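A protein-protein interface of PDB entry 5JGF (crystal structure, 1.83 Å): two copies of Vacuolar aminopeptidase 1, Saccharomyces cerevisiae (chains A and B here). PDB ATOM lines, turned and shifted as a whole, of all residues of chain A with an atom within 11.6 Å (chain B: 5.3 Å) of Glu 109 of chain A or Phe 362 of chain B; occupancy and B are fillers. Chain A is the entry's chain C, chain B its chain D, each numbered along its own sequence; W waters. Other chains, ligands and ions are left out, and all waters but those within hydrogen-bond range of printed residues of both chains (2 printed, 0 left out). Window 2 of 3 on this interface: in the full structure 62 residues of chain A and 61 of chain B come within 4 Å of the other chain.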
ATOM      1  N   LYS A 105     -20.050  26.067 -16.743  1.00  0.00           N
ATOM      2  CA  LYS A 105     -19.427  26.007 -15.425  1.00  0.00           C
ATOM      3  C   LYS A 105     -18.518  27.228 -15.319  1.00  0.00           C
ATOM      4  O   LYS A 105     -17.847  27.589 -16.287  1.00  0.00           O
ATOM      5  CB  LYS A 105     -18.585  24.737 -15.255  1.00  0.00           C
ATOM      6  CG  LYS A 105     -19.387  23.443 -15.159  1.00  0.00           C
ATOM      7  CD  LYS A 105     -18.482  22.251 -14.890  1.00  0.00           C
ATOM      8  CE  LYS A 105     -17.827  22.323 -13.513  1.00  0.00           C
ATOM      9  NZ  LYS A 105     -18.806  22.181 -12.398  1.00  0.00           N
ATOM     10  N   ASP A 106     -18.513  27.881 -14.162  1.00  0.00           N
ATOM     11  CA  ASP A 106     -17.648  29.038 -13.984  1.00  0.00           C
ATOM     12  C   ASP A 106     -16.225  28.508 -14.067  1.00  0.00           C
ATOM     13  O   ASP A 106     -15.972  27.356 -13.708  1.00  0.00           O
ATOM     14  CB  ASP A 106     -17.848  29.679 -12.606  1.00  0.00           C
ATOM     15  CG  ASP A 106     -19.263  30.165 -12.381  1.00  0.00           C
ATOM     16  OD1 ASP A 106     -19.813  30.832 -13.279  1.00  0.00           O
ATOM     17  OD2 ASP A 106     -19.820  29.889 -11.297  1.00  0.00           O
ATOM     18  N   THR A 107     -15.301  29.331 -14.550  1.00  0.00           N
ATOM     19  CA  THR A 107     -13.914  28.899 -14.624  1.00  0.00           C
ATOM     20  C   THR A 107     -13.461  28.660 -13.190  1.00  0.00           C
ATOM     21  O   THR A 107     -13.960  29.300 -12.262  1.00  0.00           O
ATOM     22  CB  THR A 107     -13.008  29.969 -15.276  1.00  0.00           C
ATOM     23  OG1 THR A 107     -13.184  31.221 -14.604  1.00  0.00           O
ATOM     24  CG2 THR A 107     -13.346  30.130 -16.749  1.00  0.00           C
ATOM     25  N   ALA A 108     -12.533  27.727 -13.013  1.00  0.00           N
ATOM     26  CA  ALA A 108     -12.016  27.386 -11.693  1.00  0.00           C
ATOM     27  C   ALA A 108     -10.521  27.663 -11.697  1.00  0.00           C
ATOM     28  O   ALA A 108      -9.744  26.916 -12.297  1.00  0.00           O
ATOM     29  CB  ALA A 108     -12.282  25.915 -11.397  1.00  0.00           C
ATOM     30  N   GLU A 109     -10.126  28.740 -11.023  1.00  0.00           N
ATOM     31  CA  GLU A 109      -8.727  29.148 -10.973  1.00  0.00           C
ATOM     32  C   GLU A 109      -8.214  29.286 -12.403  1.00  0.00           C
ATOM     33  O   GLU A 109      -7.043  29.033 -12.682  1.00  0.00           O
ATOM     34  CB  GLU A 109      -7.880  28.121 -10.208  1.00  0.00           C
ATOM     35  CG  GLU A 109      -8.249  27.937  -8.738  1.00  0.00           C
ATOM     36  CD  GLU A 109      -8.212  29.234  -7.939  1.00  0.00           C
ATOM     37  OE1 GLU A 109      -7.421  30.137  -8.286  1.00  0.00           O
ATOM     38  OE2 GLU A 109      -8.969  29.341  -6.950  1.00  0.00           O
ATOM     39  N   GLY A 110      -9.108  29.672 -13.312  1.00  0.00           N
ATOM     40  CA  GLY A 110      -8.726  29.856 -14.702  1.00  0.00           C
ATOM     41  C   GLY A 110      -9.045  28.701 -15.638  1.00  0.00           C
ATOM     42  O   GLY A 110      -9.060  28.871 -16.858  1.00  0.00           O
ATOM     43  N   TYR A 111      -9.294  27.523 -15.075  1.00  0.00           N
ATOM     44  CA  TYR A 111      -9.603  26.341 -15.880  1.00  0.00           C
ATOM     45  C   TYR A 111     -11.027  26.312 -16.391  1.00  0.00           C
ATOM     46  O   TYR A 111     -11.967  26.591 -15.650  1.00  0.00           O
ATOM     47  CB  TYR A 111      -9.379  25.069 -15.072  1.00  0.00           C
ATOM     48  CG  TYR A 111      -7.942  24.640 -14.960  1.00  0.00           C
ATOM     49  CD1 TYR A 111      -7.354  23.840 -15.939  1.00  0.00           C
ATOM     50  CD2 TYR A 111      -7.175  25.005 -13.857  1.00  0.00           C
ATOM     51  CE1 TYR A 111      -6.033  23.406 -15.812  1.00  0.00           C
ATOM     52  CE2 TYR A 111      -5.860  24.581 -13.723  1.00  0.00           C
ATOM     53  CZ  TYR A 111      -5.298  23.780 -14.699  1.00  0.00           C
ATOM     54  OH  TYR A 111      -4.008  23.331 -14.532  1.00  0.00           O
ATOM     55  N   GLY A 112     -11.174  25.955 -17.662  1.00  0.00           N
ATOM     56  CA  GLY A 112     -12.489  25.842 -18.252  1.00  0.00           C
ATOM     57  C   GLY A 112     -12.910  24.385 -18.147  1.00  0.00           C
ATOM     58  O   GLY A 112     -12.118  23.480 -18.440  1.00  0.00           O
ATOM     59  N   ARG A 113     -14.140  24.156 -17.701  1.00  0.00           N
ATOM     60  CA  ARG A 113     -14.678  22.807 -17.565  1.00  0.00           C
ATOM     61  C   ARG A 113     -16.116  22.798 -18.073  1.00  0.00           C
ATOM     62  O   ARG A 113     -16.752  23.845 -18.166  1.00  0.00           O
ATOM     63  CB  ARG A 113     -14.670  22.365 -16.097  1.00  0.00           C
ATOM     64  CG  ARG A 113     -13.286  22.206 -15.477  1.00  0.00           C
ATOM     65  CD  ARG A 113     -13.393  21.743 -14.028  1.00  0.00           C
ATOM     66  NE  ARG A 113     -14.051  22.738 -13.181  1.00  0.00           N
ATOM     67  CZ  ARG A 113     -14.346  22.549 -11.898  1.00  0.00           C
ATOM     68  NH1 ARG A 113     -14.044  21.400 -11.308  1.00  0.00           N
ATOM     69  NH2 ARG A 113     -14.942  23.510 -11.203  1.00  0.00           N
ATOM     70  N   LEU A 166      -5.637  12.579 -10.622  1.00  0.00           N
ATOM     71  CA  LEU A 166      -4.819  13.319  -9.667  1.00  0.00           C
ATOM     72  C   LEU A 166      -3.539  12.513  -9.468  1.00  0.00           C
ATOM     73  O   LEU A 166      -3.591  11.290  -9.337  1.00  0.00           O
ATOM     74  CB  LEU A 166      -5.547  13.453  -8.329  1.00  0.00           C
ATOM     75  CG  LEU A 166      -4.766  14.169  -7.220  1.00  0.00           C
ATOM     76  CD1 LEU A 166      -4.514  15.614  -7.625  1.00  0.00           C
ATOM     77  CD2 LEU A 166      -5.551  14.122  -5.918  1.00  0.00           C
ATOM     78  N   PHE A 170      -0.150  12.793  -4.079  1.00  0.00           N
ATOM     79  CA  PHE A 170      -1.027  13.376  -3.070  1.00  0.00           C
ATOM     80  C   PHE A 170      -1.644  12.389  -2.083  1.00  0.00           C
ATOM     81  O   PHE A 170      -2.339  12.792  -1.149  1.00  0.00           O
ATOM     82  CB  PHE A 170      -2.113  14.195  -3.760  1.00  0.00           C
ATOM     83  CG  PHE A 170      -1.585  15.412  -4.457  1.00  0.00           C
ATOM     84  CD1 PHE A 170      -1.307  16.571  -3.742  1.00  0.00           C
ATOM     85  CD2 PHE A 170      -1.332  15.391  -5.824  1.00  0.00           C
ATOM     86  CE1 PHE A 170      -0.784  17.697  -4.382  1.00  0.00           C
ATOM     87  CE2 PHE A 170      -0.810  16.509  -6.472  1.00  0.00           C
ATOM     88  CZ  PHE A 170      -0.536  17.664  -5.748  1.00  0.00           C
ATOM     89  N   VAL A 187     -11.979  18.760 -18.408  1.00  0.00           N
ATOM     90  CA  VAL A 187     -11.332  20.066 -18.471  1.00  0.00           C
ATOM     91  C   VAL A 187     -11.269  20.369 -19.965  1.00  0.00           C
ATOM     92  O   VAL A 187     -10.770  19.556 -20.748  1.00  0.00           O
ATOM     93  CB  VAL A 187      -9.906  20.026 -17.890  1.00  0.00           C
ATOM     94  CG1 VAL A 187      -9.171  21.328 -18.223  1.00  0.00           C
ATOM     95  CG2 VAL A 187      -9.970  19.834 -16.388  1.00  0.00           C
ATOM     96  N   GLY A 189     -10.272  23.702 -21.261  1.00  0.00           N
ATOM     97  CA  GLY A 189      -9.314  24.731 -21.625  1.00  0.00           C
ATOM     98  C   GLY A 189      -8.822  25.599 -20.487  1.00  0.00           C
ATOM     99  O   GLY A 189      -9.134  25.363 -19.322  1.00  0.00           O
ATOM    100  N   PHE A 190      -8.018  26.597 -20.838  1.00  0.00           N
ATOM    101  CA  PHE A 190      -7.481  27.556 -19.880  1.00  0.00           C
ATOM    102  C   PHE A 190      -7.309  28.831 -20.697  1.00  0.00           C
ATOM    103  O   PHE A 190      -6.229  29.110 -21.214  1.00  0.00           O
ATOM    104  CB  PHE A 190      -6.125  27.103 -19.326  1.00  0.00           C
ATOM    105  CG  PHE A 190      -5.745  27.787 -18.039  1.00  0.00           C
ATOM    106  CD1 PHE A 190      -6.101  27.238 -16.813  1.00  0.00           C
ATOM    107  CD2 PHE A 190      -5.091  29.017 -18.056  1.00  0.00           C
ATOM    108  CE1 PHE A 190      -5.816  27.901 -15.620  1.00  0.00           C
ATOM    109  CE2 PHE A 190      -4.802  29.689 -16.866  1.00  0.00           C
ATOM    110  CZ  PHE A 190      -5.168  29.128 -15.646  1.00  0.00           C
ATOM    111  N   PRO A 191      -8.389  29.611 -20.839  1.00  0.00           N
ATOM    112  CA  PRO A 191      -8.376  30.860 -21.606  1.00  0.00           C
ATOM    113  C   PRO A 191      -7.505  31.976 -21.045  1.00  0.00           C
ATOM    114  O   PRO A 191      -7.161  31.983 -19.866  1.00  0.00           O
ATOM    115  CB  PRO A 191      -9.850  31.246 -21.652  1.00  0.00           C
ATOM    116  CG  PRO A 191     -10.360  30.745 -20.343  1.00  0.00           C
ATOM    117  CD  PRO A 191      -9.718  29.377 -20.243  1.00  0.00           C
ATOM    118  N   THR A 192      -7.152  32.912 -21.917  1.00  0.00           N
ATOM    119  CA  THR A 192      -6.339  34.061 -21.542  1.00  0.00           C
ATOM    120  C   THR A 192      -7.079  35.311 -22.008  1.00  0.00           C
ATOM    121  O   THR A 192      -7.849  35.260 -22.965  1.00  0.00           O
ATOM    122  CB  THR A 192      -4.950  34.008 -22.216  1.00  0.00           C
ATOM    123  OG1 THR A 192      -5.108  33.897 -23.636  1.00  0.00           O
ATOM    124  CG2 THR A 192      -4.158  32.815 -21.705  1.00  0.00           C
ATOM    125  N   PRO A 193      -6.864  36.451 -21.331  1.00  0.00           N
ATOM    126  CA  PRO A 193      -7.539  37.694 -21.718  1.00  0.00           C
ATOM    127  C   PRO A 193      -7.043  38.247 -23.052  1.00  0.00           C
ATOM    128  O   PRO A 193      -7.596  37.935 -24.108  1.00  0.00           O
ATOM    129  CB  PRO A 193      -7.231  38.625 -20.551  1.00  0.00           C
ATOM    130  CG  PRO A 193      -5.865  38.177 -20.136  1.00  0.00           C
ATOM    131  CD  PRO A 193      -5.989  36.670 -20.165  1.00  0.00           C
ATOM    132  N   HIS B 347       3.483  19.766  -9.882  1.00  0.00           N
ATOM    133  CA  HIS B 347       2.051  19.647 -10.127  1.00  0.00           C
ATOM    134  C   HIS B 347       1.217  20.853 -10.516  1.00  0.00           C
ATOM    135  O   HIS B 347       1.128  21.827  -9.772  1.00  0.00           O
ATOM    136  CB  HIS B 347       1.397  19.004  -8.902  1.00  0.00           C
ATOM    137  CG  HIS B 347       2.064  17.743  -8.452  1.00  0.00           C
ATOM    138  ND1 HIS B 347       1.923  16.546  -9.120  1.00  0.00           N
ATOM    139  CD2 HIS B 347       2.885  17.495  -7.403  1.00  0.00           C
ATOM    140  CE1 HIS B 347       2.628  15.614  -8.503  1.00  0.00           C
ATOM    141  NE2 HIS B 347       3.222  16.164  -7.459  1.00  0.00           N
ATOM    142  N   TYR B 349      -2.217  22.809 -10.990  1.00  0.00           N
ATOM    143  CA  TYR B 349      -3.451  22.797 -10.225  1.00  0.00           C
ATOM    144  C   TYR B 349      -4.465  21.941 -10.984  1.00  0.00           C
ATOM    145  O   TYR B 349      -4.662  22.131 -12.183  1.00  0.00           O
ATOM    146  CB  TYR B 349      -3.995  24.220 -10.112  1.00  0.00           C
ATOM    147  CG  TYR B 349      -5.303  24.332  -9.361  1.00  0.00           C
ATOM    148  CD1 TYR B 349      -5.343  24.225  -7.972  1.00  0.00           C
ATOM    149  CD2 TYR B 349      -6.500  24.561 -10.040  1.00  0.00           C
ATOM    150  CE1 TYR B 349      -6.549  24.349  -7.272  1.00  0.00           C
ATOM    151  CE2 TYR B 349      -7.708  24.686  -9.351  1.00  0.00           C
ATOM    152  CZ  TYR B 349      -7.723  24.580  -7.969  1.00  0.00           C
ATOM    153  OH  TYR B 349      -8.909  24.711  -7.283  1.00  0.00           O
ATOM    154  N   TYR B 357      -4.568  21.166  -3.118  1.00  0.00           N
ATOM    155  CA  TYR B 357      -3.649  22.208  -3.550  1.00  0.00           C
ATOM    156  C   TYR B 357      -3.628  23.383  -2.581  1.00  0.00           C
ATOM    157  O   TYR B 357      -4.670  23.847  -2.117  1.00  0.00           O
ATOM    158  CB  TYR B 357      -3.995  22.680  -4.962  1.00  0.00           C
ATOM    159  CG  TYR B 357      -3.637  21.666  -6.028  1.00  0.00           C
ATOM    160  CD1 TYR B 357      -4.534  20.661  -6.400  1.00  0.00           C
ATOM    161  CD2 TYR B 357      -2.382  21.685  -6.639  1.00  0.00           C
ATOM    162  CE1 TYR B 357      -4.187  19.701  -7.358  1.00  0.00           C
ATOM    163  CE2 TYR B 357      -2.026  20.732  -7.595  1.00  0.00           C
ATOM    164  CZ  TYR B 357      -2.933  19.744  -7.949  1.00  0.00           C
ATOM    165  OH  TYR B 357      -2.582  18.809  -8.900  1.00  0.00           O
ATOM    166  N   LEU B 358      -2.424  23.853  -2.281  1.00  0.00           N
ATOM    167  CA  LEU B 358      -2.223  24.956  -1.347  1.00  0.00           C
ATOM    168  C   LEU B 358      -2.486  26.313  -1.988  1.00  0.00           C
ATOM    169  O   LEU B 358      -1.836  26.689  -2.965  1.00  0.00           O
ATOM    170  CB  LEU B 358      -0.792  24.907  -0.804  1.00  0.00           C
ATOM    171  CG  LEU B 358      -0.356  26.006   0.170  1.00  0.00           C
ATOM    172  CD1 LEU B 358      -1.205  25.951   1.438  1.00  0.00           C
ATOM    173  CD2 LEU B 358       1.116  25.813   0.507  1.00  0.00           C
ATOM    174  N   LYS B 359      -3.445  27.044  -1.428  1.00  0.00           N
ATOM    175  CA  LYS B 359      -3.797  28.360  -1.936  1.00  0.00           C
ATOM    176  C   LYS B 359      -2.544  29.224  -2.034  1.00  0.00           C
ATOM    177  O   LYS B 359      -1.726  29.252  -1.113  1.00  0.00           O
ATOM    178  CB  LYS B 359      -4.822  29.022  -1.011  1.00  0.00           C
ATOM    179  CG  LYS B 359      -5.355  30.353  -1.517  1.00  0.00           C
ATOM    180  CD  LYS B 359      -6.472  30.868  -0.621  1.00  0.00           C
ATOM    181  CE  LYS B 359      -7.018  32.196  -1.129  1.00  0.00           C
ATOM    182  NZ  LYS B 359      -7.546  32.076  -2.514  1.00  0.00           N
ATOM    183  N   ASN B 360      -2.412  29.916  -3.162  1.00  0.00           N
ATOM    184  CA  ASN B 360      -1.277  30.791  -3.450  1.00  0.00           C
ATOM    185  C   ASN B 360       0.025  30.044  -3.708  1.00  0.00           C
ATOM    186  O   ASN B 360       1.074  30.669  -3.884  1.00  0.00           O
ATOM    187  CB  ASN B 360      -1.067  31.807  -2.322  1.00  0.00           C
ATOM    188  CG  ASN B 360      -2.238  32.758  -2.176  1.00  0.00           C
ATOM    189  OD1 ASN B 360      -2.783  33.239  -3.171  1.00  0.00           O
ATOM    190  ND2 ASN B 360      -2.622  33.043  -0.937  1.00  0.00           N
ATOM    191  N   HIS B 361      -0.041  28.713  -3.734  1.00  0.00           N
ATOM    192  CA  HIS B 361       1.148  27.900  -3.980  1.00  0.00           C
ATOM    193  C   HIS B 361       0.929  26.781  -4.995  1.00  0.00           C
ATOM    194  O   HIS B 361       1.309  25.632  -4.763  1.00  0.00           O
ATOM    195  CB  HIS B 361       1.683  27.289  -2.680  1.00  0.00           C
ATOM    196  CG  HIS B 361       2.078  28.298  -1.648  1.00  0.00           C
ATOM    197  ND1 HIS B 361       1.157  28.992  -0.894  1.00  0.00           N
ATOM    198  CD2 HIS B 361       3.297  28.716  -1.230  1.00  0.00           C
ATOM    199  CE1 HIS B 361       1.790  29.791  -0.053  1.00  0.00           C
ATOM    200  NE2 HIS B 361       3.090  29.643  -0.237  1.00  0.00           N
ATOM    201  N   PHE B 362       0.292  27.111  -6.111  1.00  0.00           N
ATOM    202  CA  PHE B 362       0.095  26.140  -7.174  1.00  0.00           C
ATOM    203  C   PHE B 362       0.219  26.865  -8.505  1.00  0.00           C
ATOM    204  O   PHE B 362      -0.105  28.050  -8.612  1.00  0.00           O
ATOM    205  CB  PHE B 362      -1.263  25.421  -7.055  1.00  0.00           C
ATOM    206  CG  PHE B 362      -2.460  26.333  -7.118  1.00  0.00           C
ATOM    207  CD1 PHE B 362      -2.838  26.933  -8.315  1.00  0.00           C
ATOM    208  CD2 PHE B 362      -3.222  26.571  -5.977  1.00  0.00           C
ATOM    209  CE1 PHE B 362      -3.963  27.758  -8.379  1.00  0.00           C
ATOM    210  CE2 PHE B 362      -4.352  27.394  -6.029  1.00  0.00           C
ATOM    211  CZ  PHE B 362      -4.722  27.987  -7.231  1.00  0.00           C
ATOM    212  N   PRO B 363       0.737  26.171  -9.528  1.00  0.00           N
ATOM    213  CA  PRO B 363       0.915  26.740 -10.864  1.00  0.00           C
ATOM    214  C   PRO B 363      -0.259  26.445 -11.792  1.00  0.00           C
ATOM    215  O   PRO B 363      -1.061  25.548 -11.536  1.00  0.00           O
ATOM    216  CB  PRO B 363       2.187  26.061 -11.342  1.00  0.00           C
ATOM    217  CG  PRO B 363       2.000  24.662 -10.808  1.00  0.00           C
ATOM    218  CD  PRO B 363       1.477  24.901  -9.396  1.00  0.00           C
ATOM    219  N   VAL B 364      -0.350  27.217 -12.868  1.00  0.00           N
ATOM    220  CA  VAL B 364      -1.390  27.028 -13.866  1.00  0.00           C
ATOM    221  C   VAL B 364      -0.678  26.884 -15.207  1.00  0.00           C
ATOM    222  O   VAL B 364       0.517  27.164 -15.315  1.00  0.00           O
ATOM    223  CB  VAL B 364      -2.380  28.212 -13.891  1.00  0.00           C
ATOM    224  CG1 VAL B 364      -3.087  28.308 -12.539  1.00  0.00           C
ATOM    225  CG2 VAL B 364      -1.653  29.512 -14.206  1.00  0.00           C
ATOM    226  N   GLN B 401       6.266  30.641 -11.081  1.00  0.00           N
ATOM    227  CA  GLN B 401       5.125  30.199 -10.285  1.00  0.00           C
ATOM    228  C   GLN B 401       5.634  29.423  -9.081  1.00  0.00           C
ATOM    229  O   GLN B 401       6.818  29.104  -8.998  1.00  0.00           O
ATOM    230  CB  GLN B 401       4.205  29.308 -11.117  1.00  0.00           C
ATOM    231  CG  GLN B 401       3.841  29.889 -12.469  1.00  0.00           C
ATOM    232  CD  GLN B 401       2.711  29.128 -13.123  1.00  0.00           C
ATOM    233  OE1 GLN B 401       1.544  29.316 -12.780  1.00  0.00           O
ATOM    234  NE2 GLN B 401       3.053  28.253 -14.061  1.00  0.00           N
ATOM    235  N   TYR B 402       4.733  29.115  -8.155  1.00  0.00           N
ATOM    236  CA  TYR B 402       5.099  28.388  -6.944  1.00  0.00           C
ATOM    237  C   TYR B 402       4.313  27.103  -6.744  1.00  0.00           C
ATOM    238  O   TYR B 402       3.144  27.013  -7.117  1.00  0.00           O
ATOM    239  CB  TYR B 402       4.803  29.218  -5.694  1.00  0.00           C
ATOM    240  CG  TYR B 402       5.693  30.393  -5.379  1.00  0.00           C
ATOM    241  CD1 TYR B 402       6.868  30.641  -6.087  1.00  0.00           C
ATOM    242  CD2 TYR B 402       5.367  31.242  -4.324  1.00  0.00           C
ATOM    243  CE1 TYR B 402       7.699  31.716  -5.743  1.00  0.00           C
ATOM    244  CE2 TYR B 402       6.178  32.305  -3.973  1.00  0.00           C
ATOM    245  CZ  TYR B 402       7.340  32.539  -4.681  1.00  0.00           C
ATOM    246  OH  TYR B 402       8.136  33.596  -4.303  1.00  0.00           O
ATOM    247  N   PHE B 403       4.970  26.114  -6.145  1.00  0.00           N
ATOM    248  CA  PHE B 403       4.298  24.888  -5.752  1.00  0.00           C
ATOM    249  C   PHE B 403       4.870  24.415  -4.425  1.00  0.00           C
ATOM    250  O   PHE B 403       6.085  24.253  -4.274  1.00  0.00           O
ATOM    251  CB  PHE B 403       4.417  23.739  -6.756  1.00  0.00           C
ATOM    252  CG  PHE B 403       3.754  22.472  -6.262  1.00  0.00           C
ATOM    253  CD1 PHE B 403       4.471  21.534  -5.523  1.00  0.00           C
ATOM    254  CD2 PHE B 403       2.381  22.294  -6.408  1.00  0.00           C
ATOM    255  CE1 PHE B 403       3.828  20.442  -4.927  1.00  0.00           C
ATOM    256  CE2 PHE B 403       1.727  21.208  -5.817  1.00  0.00           C
ATOM    257  CZ  PHE B 403       2.453  20.282  -5.074  1.00  0.00           C
HETATM  258  O   HOH W   1      -8.840  26.356  -5.257  1.00  0.00           O
HETATM  259  O   HOH W   2      -7.109  29.561  -4.570  1.00  0.00           O
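Among the printed residues, 7 pairs touch across the chains.
Among the printed residues, no Asp or Glu carboxylate lies within 4 Å of a Lys or Arg side-chain nitrogen of the other chain.
Glu 109 of chain A touches just these residues of chain B: Tyr 349 (3.4 Å) and Phe 362 (3.6 Å).
Phe 362 of chain B touches just one residue of chain A: Glu 109 (3.6 Å).
Tyr 357 of chain B touches just these residues of chain A: Leu 166 and Phe 170.
His 361 of chain B touches none of the printed residues of chain A.
No residue of chain A comes within 4 Å of Pro 363 of chain B.
Val 364 of chain B touches one residue of chain A.
No residue of chain A comes within 4 Å of Gln 401 of chain B.
No residue of chain A comes within 4 Å of Phe 403 of chain B.
Printed residues of chain B within 4 Å of Phe 170 of chain A: His 347 (3.7 Å) and Tyr 357 (3.8 Å).
Of the printed residues of chain B, Leu 166 of chain A touches Tyr 357 (3.9 Å).
Printed residues of chain A within 4 Å of His 347 of chain B: Phe 170 (3.7 Å).
The nearest residue of chain B that does not touch Glu 109 of chain A is Val 364 of chain B (4.02 Å).
The backbone carbonyl oxygen (O) of Tyr 349 of chain B is in hydrogen-bond range of the side-chain hydroxyl (OH) of Tyr 111 of chain A.
Water W1 bridges OH of Tyr 349 of chain B and OE2 of Glu 109 of chain A.
Water W2 lies within hydrogen-bond range of OE2 of Glu 109 of chain A (3.0 Å) and NZ of Lys 359 of chain B (3.3 Å).
Tyr 349 of chain B touches Glu 109 of chain A (CE2 to CG, 3.4 Å).
CZ of Phe 362 of chain B touches OE1 of Glu 109 of chain A (3.6 Å).
CD1 of Leu 166 of chain A touches OH of Tyr 357 of chain B, at 3.9 Å.
Phe 170 of chain A touches His 347 of chain B.
Tyr 357 of chain B touches Phe 170 of chain A (OH to CE2, 3.8 Å).
Phe 190 of chain A touches Val 364 of chain B (CZ to CB, 3.4 Å).
No position is printed for both chains.
Of the 7 pairs that touch across the chains among the printed residues, none has its exchanged pair printed and touching as well.
O of Pro 363 of chain B lies within hydrogen-bond range of N of Tyr 349 of chain B (3.0 Å).
The backbone NH (N) of Phe 362 of chain B is in hydrogen-bond range of the backbone carbonyl oxygen (O) of Tyr 402 of chain B.
N of Val 364 of chain B is in hydrogen-bond range of OE1 of Gln 401 of chain B (2.8 Å).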
